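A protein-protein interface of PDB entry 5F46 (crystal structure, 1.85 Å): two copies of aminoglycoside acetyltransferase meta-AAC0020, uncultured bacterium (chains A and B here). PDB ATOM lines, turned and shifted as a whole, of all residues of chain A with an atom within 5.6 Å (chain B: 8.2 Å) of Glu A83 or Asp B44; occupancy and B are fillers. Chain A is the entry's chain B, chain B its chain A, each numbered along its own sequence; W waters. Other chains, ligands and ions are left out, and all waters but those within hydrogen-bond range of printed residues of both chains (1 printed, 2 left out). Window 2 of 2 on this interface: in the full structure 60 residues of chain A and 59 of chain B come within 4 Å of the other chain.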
ATOM      1  N   GLU A  78     -18.827  -9.391  26.030  1.00  0.00           N
ATOM      2  CA  GLU A  78     -19.317 -10.007  24.797  1.00  0.00           C
ATOM      3  C   GLU A  78     -20.833  -9.869  24.740  1.00  0.00           C
ATOM      4  O   GLU A  78     -21.519 -10.131  25.721  1.00  0.00           O
ATOM      5  CB  GLU A  78     -18.901 -11.477  24.715  1.00  0.00           C
ATOM      6  CG  GLU A  78     -17.444 -11.715  24.334  1.00  0.00           C
ATOM      7  CD  GLU A  78     -17.199 -11.672  22.828  1.00  0.00           C
ATOM      8  OE1 GLU A  78     -18.169 -11.523  22.049  1.00  0.00           O
ATOM      9  OE2 GLU A  78     -16.028 -11.797  22.420  1.00  0.00           O
ATOM     10  N   GLN A  79     -21.341  -9.449  23.587  1.00  0.00           N
ATOM     11  CA  GLN A  79     -22.762  -9.156  23.414  1.00  0.00           C
ATOM     12  C   GLN A  79     -23.549 -10.318  22.827  1.00  0.00           C
ATOM     13  O   GLN A  79     -22.987 -11.160  22.129  1.00  0.00           O
ATOM     14  CB  GLN A  79     -22.944  -7.952  22.494  1.00  0.00           C
ATOM     15  CG  GLN A  79     -22.748  -6.620  23.142  1.00  0.00           C
ATOM     16  CD  GLN A  79     -23.327  -5.511  22.284  1.00  0.00           C
ATOM     17  OE1 GLN A  79     -24.428  -5.032  22.543  1.00  0.00           O
ATOM     18  NE2 GLN A  79     -22.591  -5.109  21.251  1.00  0.00           N
ATOM     19  N   TYR A  81     -26.501  -9.231  21.303  1.00  0.00           N
ATOM     20  CA  TYR A  81     -27.186  -8.453  20.264  1.00  0.00           C
ATOM     21  C   TYR A  81     -26.330  -8.332  19.010  1.00  0.00           C
ATOM     22  O   TYR A  81     -26.823  -7.998  17.933  1.00  0.00           O
ATOM     23  CB  TYR A  81     -27.525  -7.047  20.766  1.00  0.00           C
ATOM     24  CG  TYR A  81     -28.547  -6.989  21.876  1.00  0.00           C
ATOM     25  CD1 TYR A  81     -29.719  -7.735  21.817  1.00  0.00           C
ATOM     26  CD2 TYR A  81     -28.331  -6.191  22.991  1.00  0.00           C
ATOM     27  CE1 TYR A  81     -30.652  -7.674  22.838  1.00  0.00           C
ATOM     28  CE2 TYR A  81     -29.251  -6.125  24.011  1.00  0.00           C
ATOM     29  CZ  TYR A  81     -30.409  -6.866  23.933  1.00  0.00           C
ATOM     30  OH  TYR A  81     -31.320  -6.795  24.958  1.00  0.00           O
ATOM     31  N   SER A  82     -25.036  -8.590  19.161  1.00  0.00           N
ATOM     32  CA  SER A  82     -24.084  -8.387  18.078  1.00  0.00           C
ATOM     33  C   SER A  82     -22.832  -9.209  18.330  1.00  0.00           C
ATOM     34  O   SER A  82     -22.544  -9.562  19.472  1.00  0.00           O
ATOM     35  CB  SER A  82     -23.723  -6.904  17.953  1.00  0.00           C
ATOM     36  OG  SER A  82     -22.638  -6.713  17.062  1.00  0.00           O
ATOM     37  N   GLU A  83     -22.089  -9.510  17.268  1.00  0.00           N
ATOM     38  CA  GLU A  83     -20.800 -10.177  17.431  1.00  0.00           C
ATOM     39  C   GLU A  83     -19.707  -9.180  17.815  1.00  0.00           C
ATOM     40  O   GLU A  83     -18.588  -9.574  18.132  1.00  0.00           O
ATOM     41  CB  GLU A  83     -20.405 -10.926  16.155  1.00  0.00           C
ATOM     42  CG  GLU A  83     -21.296 -12.120  15.846  1.00  0.00           C
ATOM     43  CD  GLU A  83     -20.713 -13.040  14.784  1.00  0.00           C
ATOM     44  OE1 GLU A  83     -19.485 -12.998  14.564  1.00  0.00           O
ATOM     45  OE2 GLU A  83     -21.487 -13.813  14.178  1.00  0.00           O
ATOM     46  N   LYS A  84     -20.032  -7.890  17.782  1.00  0.00           N
ATOM     47  CA  LYS A  84     -19.089  -6.855  18.206  1.00  0.00           C
ATOM     48  C   LYS A  84     -19.252  -6.569  19.697  1.00  0.00           C
ATOM     49  O   LYS A  84     -20.299  -6.095  20.132  1.00  0.00           O
ATOM     50  CB  LYS A  84     -19.285  -5.573  17.395  1.00  0.00           C
ATOM     51  CG  LYS A  84     -19.253  -5.784  15.890  1.00  0.00           C
ATOM     52  CD  LYS A  84     -19.028  -4.486  15.133  1.00  0.00           C
ATOM     53  CE  LYS A  84     -20.092  -3.452  15.454  1.00  0.00           C
ATOM     54  NZ  LYS A  84     -19.819  -2.160  14.758  1.00  0.00           N
ATOM     55  N   PRO A  85     -18.209  -6.859  20.488  1.00  0.00           N
ATOM     56  CA  PRO A  85     -18.296  -6.708  21.945  1.00  0.00           C
ATOM     57  C   PRO A  85     -18.435  -5.260  22.403  1.00  0.00           C
ATOM     58  O   PRO A  85     -18.254  -4.325  21.621  1.00  0.00           O
ATOM     59  CB  PRO A  85     -16.965  -7.288  22.446  1.00  0.00           C
ATOM     60  CG  PRO A  85     -16.425  -8.091  21.311  1.00  0.00           C
ATOM     61  CD  PRO A  85     -16.917  -7.418  20.064  1.00  0.00           C
ATOM     62  N   LEU B  21     -29.230 -23.094  24.612  1.00  0.00           N
ATOM     63  CA  LEU B  21     -29.256 -22.080  23.560  1.00  0.00           C
ATOM     64  C   LEU B  21     -30.683 -21.708  23.096  1.00  0.00           C
ATOM     65  O   LEU B  21     -30.967 -20.524  22.917  1.00  0.00           O
ATOM     66  CB  LEU B  21     -28.412 -22.534  22.363  1.00  0.00           C
ATOM     67  CG  LEU B  21     -28.250 -21.539  21.211  1.00  0.00           C
ATOM     68  CD1 LEU B  21     -27.514 -20.292  21.669  1.00  0.00           C
ATOM     69  CD2 LEU B  21     -27.538 -22.187  20.026  1.00  0.00           C
ATOM     70  N   ILE B  25     -32.093 -17.885  23.152  1.00  0.00           N
ATOM     71  CA  ILE B  25     -32.616 -17.185  21.990  1.00  0.00           C
ATOM     72  C   ILE B  25     -34.024 -16.672  22.272  1.00  0.00           C
ATOM     73  O   ILE B  25     -34.396 -15.576  21.851  1.00  0.00           O
ATOM     74  CB  ILE B  25     -32.608 -18.105  20.753  1.00  0.00           C
ATOM     75  CG1 ILE B  25     -31.159 -18.424  20.369  1.00  0.00           C
ATOM     76  CG2 ILE B  25     -33.358 -17.469  19.590  1.00  0.00           C
ATOM     77  CD1 ILE B  25     -31.016 -19.404  19.238  1.00  0.00           C
ATOM     78  N   ILE B  28     -33.653 -13.550  24.239  1.00  0.00           N
ATOM     79  CA  ILE B  28     -33.205 -12.472  23.366  1.00  0.00           C
ATOM     80  C   ILE B  28     -34.387 -11.927  22.565  1.00  0.00           C
ATOM     81  O   ILE B  28     -34.536 -10.711  22.403  1.00  0.00           O
ATOM     82  CB  ILE B  28     -32.090 -12.945  22.413  1.00  0.00           C
ATOM     83  CG1 ILE B  28     -30.866 -13.398  23.211  1.00  0.00           C
ATOM     84  CG2 ILE B  28     -31.703 -11.835  21.447  1.00  0.00           C
ATOM     85  CD1 ILE B  28     -29.765 -13.974  22.362  1.00  0.00           C
ATOM     86  N   SER B  41     -31.128  -7.874  14.016  1.00  0.00           N
ATOM     87  CA  SER B  41     -30.705  -9.121  13.391  1.00  0.00           C
ATOM     88  C   SER B  41     -29.927  -9.936  14.407  1.00  0.00           C
ATOM     89  O   SER B  41     -28.834  -9.546  14.816  1.00  0.00           O
ATOM     90  CB  SER B  41     -29.855  -8.858  12.146  1.00  0.00           C
ATOM     91  OG  SER B  41     -30.597  -8.170  11.154  1.00  0.00           O
ATOM     92  N   ILE B  42     -30.495 -11.061  14.824  1.00  0.00           N
ATOM     93  CA  ILE B  42     -29.881 -11.872  15.869  1.00  0.00           C
ATOM     94  C   ILE B  42     -28.564 -12.467  15.363  1.00  0.00           C
ATOM     95  O   ILE B  42     -28.449 -12.839  14.198  1.00  0.00           O
ATOM     96  CB  ILE B  42     -30.854 -12.987  16.353  1.00  0.00           C
ATOM     97  CG1 ILE B  42     -30.407 -13.563  17.700  1.00  0.00           C
ATOM     98  CG2 ILE B  42     -31.036 -14.069  15.294  1.00  0.00           C
ATOM     99  CD1 ILE B  42     -31.443 -14.431  18.364  1.00  0.00           C
ATOM    100  N   PRO B  43     -27.538 -12.501  16.227  1.00  0.00           N
ATOM    101  CA  PRO B  43     -26.263 -13.090  15.803  1.00  0.00           C
ATOM    102  C   PRO B  43     -26.380 -14.588  15.550  1.00  0.00           C
ATOM    103  O   PRO B  43     -27.334 -15.216  16.017  1.00  0.00           O
ATOM    104  CB  PRO B  43     -25.334 -12.815  16.989  1.00  0.00           C
ATOM    105  CG  PRO B  43     -25.948 -11.655  17.695  1.00  0.00           C
ATOM    106  CD  PRO B  43     -27.429 -11.822  17.528  1.00  0.00           C
ATOM    107  N   ASP B  44     -25.415 -15.144  14.824  1.00  0.00           N
ATOM    108  CA  ASP B  44     -25.373 -16.578  14.566  1.00  0.00           C
ATOM    109  C   ASP B  44     -25.364 -17.362  15.869  1.00  0.00           C
ATOM    110  O   ASP B  44     -24.912 -16.869  16.905  1.00  0.00           O
ATOM    111  CB  ASP B  44     -24.145 -16.942  13.732  1.00  0.00           C
ATOM    112  CG  ASP B  44     -24.137 -16.259  12.383  1.00  0.00           C
ATOM    113  OD1 ASP B  44     -25.231 -15.973  11.853  1.00  0.00           O
ATOM    114  OD2 ASP B  44     -23.034 -16.010  11.852  1.00  0.00           O
ATOM    115  N   SER B  45     -25.872 -18.587  15.812  1.00  0.00           N
ATOM    116  CA  SER B  45     -25.981 -19.416  17.003  1.00  0.00           C
ATOM    117  C   SER B  45     -24.610 -19.838  17.513  1.00  0.00           C
ATOM    118  O   SER B  45     -24.435 -20.092  18.702  1.00  0.00           O
ATOM    119  CB  SER B  45     -26.845 -20.643  16.715  1.00  0.00           C
ATOM    120  OG  SER B  45     -28.153 -20.242  16.357  1.00  0.00           O
ATOM    121  N   GLU B  46     -23.642 -19.905  16.602  1.00  0.00           N
ATOM    122  CA  GLU B  46     -22.265 -20.204  16.972  1.00  0.00           C
ATOM    123  C   GLU B  46     -21.757 -19.180  17.984  1.00  0.00           C
ATOM    124  O   GLU B  46     -21.169 -19.537  19.006  1.00  0.00           O
ATOM    125  CB  GLU B  46     -21.372 -20.221  15.732  1.00  0.00           C
ATOM    126  CG  GLU B  46     -19.912 -20.516  16.010  1.00  0.00           C
ATOM    127  CD  GLU B  46     -19.085 -20.581  14.739  1.00  0.00           C
ATOM    128  OE1 GLU B  46     -19.643 -20.326  13.650  1.00  0.00           O
ATOM    129  OE2 GLU B  46     -17.879 -20.892  14.828  1.00  0.00           O
ATOM    130  N   HIS B  47     -22.007 -17.907  17.699  1.00  0.00           N
ATOM    131  CA  HIS B  47     -21.585 -16.831  18.588  1.00  0.00           C
ATOM    132  C   HIS B  47     -22.321 -16.891  19.920  1.00  0.00           C
ATOM    133  O   HIS B  47     -21.711 -16.800  20.986  1.00  0.00           O
ATOM    134  CB  HIS B  47     -21.811 -15.471  17.931  1.00  0.00           C
ATOM    135  CG  HIS B  47     -21.529 -14.317  18.835  1.00  0.00           C
ATOM    136  ND1 HIS B  47     -20.245 -13.890  19.119  1.00  0.00           N
ATOM    137  CD2 HIS B  47     -22.352 -13.509  19.539  1.00  0.00           C
ATOM    138  CE1 HIS B  47     -20.297 -12.867  19.947  1.00  0.00           C
ATOM    139  NE2 HIS B  47     -21.567 -12.614  20.221  1.00  0.00           N
ATOM    140  N   LEU B  48     -23.640 -17.049  19.851  1.00  0.00           N
ATOM    141  CA  LEU B  48     -24.466 -17.086  21.052  1.00  0.00           C
ATOM    142  C   LEU B  48     -24.120 -18.285  21.934  1.00  0.00           C
ATOM    143  O   LEU B  48     -24.164 -18.191  23.161  1.00  0.00           O
ATOM    144  CB  LEU B  48     -25.952 -17.113  20.680  1.00  0.00           C
ATOM    145  CG  LEU B  48     -26.490 -15.866  19.968  1.00  0.00           C
ATOM    146  CD1 LEU B  48     -27.984 -16.007  19.650  1.00  0.00           C
ATOM    147  CD2 LEU B  48     -26.225 -14.621  20.804  1.00  0.00           C
ATOM    148  N   GLN B  49     -23.777 -19.405  21.308  1.00  0.00           N
ATOM    149  CA  GLN B  49     -23.396 -20.604  22.050  1.00  0.00           C
ATOM    150  C   GLN B  49     -22.115 -20.383  22.841  1.00  0.00           C
ATOM    151  O   GLN B  49     -22.008 -20.790  24.001  1.00  0.00           O
ATOM    152  CB  GLN B  49     -23.226 -21.796  21.103  1.00  0.00           C
ATOM    153  CG  GLN B  49     -22.851 -23.099  21.803  1.00  0.00           C
ATOM    154  CD  GLN B  49     -23.920 -23.565  22.772  1.00  0.00           C
ATOM    155  OE1 GLN B  49     -24.907 -24.181  22.370  1.00  0.00           O
ATOM    156  NE2 GLN B  49     -23.735 -23.266  24.054  1.00  0.00           N
ATOM    157  N   LYS B  50     -21.144 -19.730  22.214  1.00  0.00           N
ATOM    158  CA  LYS B  50     -19.851 -19.536  22.854  1.00  0.00           C
ATOM    159  C   LYS B  50     -20.012 -18.567  24.023  1.00  0.00           C
ATOM    160  O   LYS B  50     -19.431 -18.767  25.095  1.00  0.00           O
ATOM    161  CB  LYS B  50     -18.822 -19.031  21.848  1.00  0.00           C
ATOM    162  CG  LYS B  50     -17.738 -18.132  22.405  1.00  0.00           C
ATOM    163  CD  LYS B  50     -16.819 -17.620  21.300  1.00  0.00           C
ATOM    164  CE  LYS B  50     -15.550 -17.004  21.872  1.00  0.00           C
ATOM    165  NZ  LYS B  50     -15.397 -15.557  21.560  1.00  0.00           N
ATOM    166  N   LEU B  51     -20.831 -17.536  23.832  1.00  0.00           N
ATOM    167  CA  LEU B  51     -21.145 -16.602  24.913  1.00  0.00           C
ATOM    168  C   LEU B  51     -21.827 -17.303  26.088  1.00  0.00           C
ATOM    169  O   LEU B  51     -21.500 -17.046  27.248  1.00  0.00           O
ATOM    170  CB  LEU B  51     -22.027 -15.470  24.392  1.00  0.00           C
ATOM    171  CG  LEU B  51     -22.578 -14.525  25.457  1.00  0.00           C
ATOM    172  CD1 LEU B  51     -21.445 -13.899  26.267  1.00  0.00           C
ATOM    173  CD2 LEU B  51     -23.458 -13.450  24.833  1.00  0.00           C
HETATM  174  O   HOH W   1     -23.701 -13.008  13.640  1.00  0.00           O
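A ring nitrogen (NE2) of His B47 sits at hydrogen-bond distance from the backbone carbonyl oxygen (O) of Gln A79, at 2.8 Å.
O of Ser A82 is in hydrogen-bond range of NE2 of His B47, 3.3 Å away.
The side-chain amino group of Lys B50 lies within salt-bridge range of the side-chain carboxylate of Glu A78, 3.9 Å away.
NE2 of Gln A79 sits at hydrogen-bond distance from O of Lys A84.
OG of Ser A82 sits at hydrogen-bond distance from N of Lys A84, 2.9 Å away.
Among the printed residues, pairs that only touch across the chains: Glu A78 with His B47, Glu A78 with Leu B51, Gln A79 with Leu B51, Tyr A81 with Pro B43, Ser A82 with Pro B43, Glu A83 with Asp B44 and Glu A83 with His B47.
Of the printed residues of chain B, Glu A78 touches His B47, Lys B50 and Leu B51.
Printed residues of chain B within 4 Å of Gln A79: His B47 and Leu B51.
Of the printed residues of chain B, Tyr A81 touches Pro B43.
Of chain B, only Pro B43 (3.5 Å) and His B47 (3.3 Å) come within 4 Å of Ser A82.
Of chain B, only Asp B44 and His B47 come within 4 Å of Glu A83.
Ile B28 touches none of the printed residues of chain A.
Printed residues of chain A within 4 Å of Pro B43: Tyr A81 and Ser A82.
Printed residues of chain A within 4 Å of His B47: Glu A78 (3.3 Å), Gln A79 (2.8 Å), Ser A82 (3.3 Å) and Glu A83 (3.7 Å).
Leu B48 touches none of the printed residues of chain A.
Among the printed residues, 10 pairs touch across the chains.
Among the printed residues, Asp or Glu carboxylates within 4 Å of a Lys or Arg side-chain nitrogen of the other chain: Glu A78 with Lys B50 (3.9 Å).
No position is printed for both chains.
Of the 10 pairs that touch across the chains among the printed residues, none has its exchanged pair printed and touching as well.
Water W1 lies within hydrogen-bond range of OE2 of Glu A83 (2.4 Å) and N of Asp B44 (3.0 Å).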
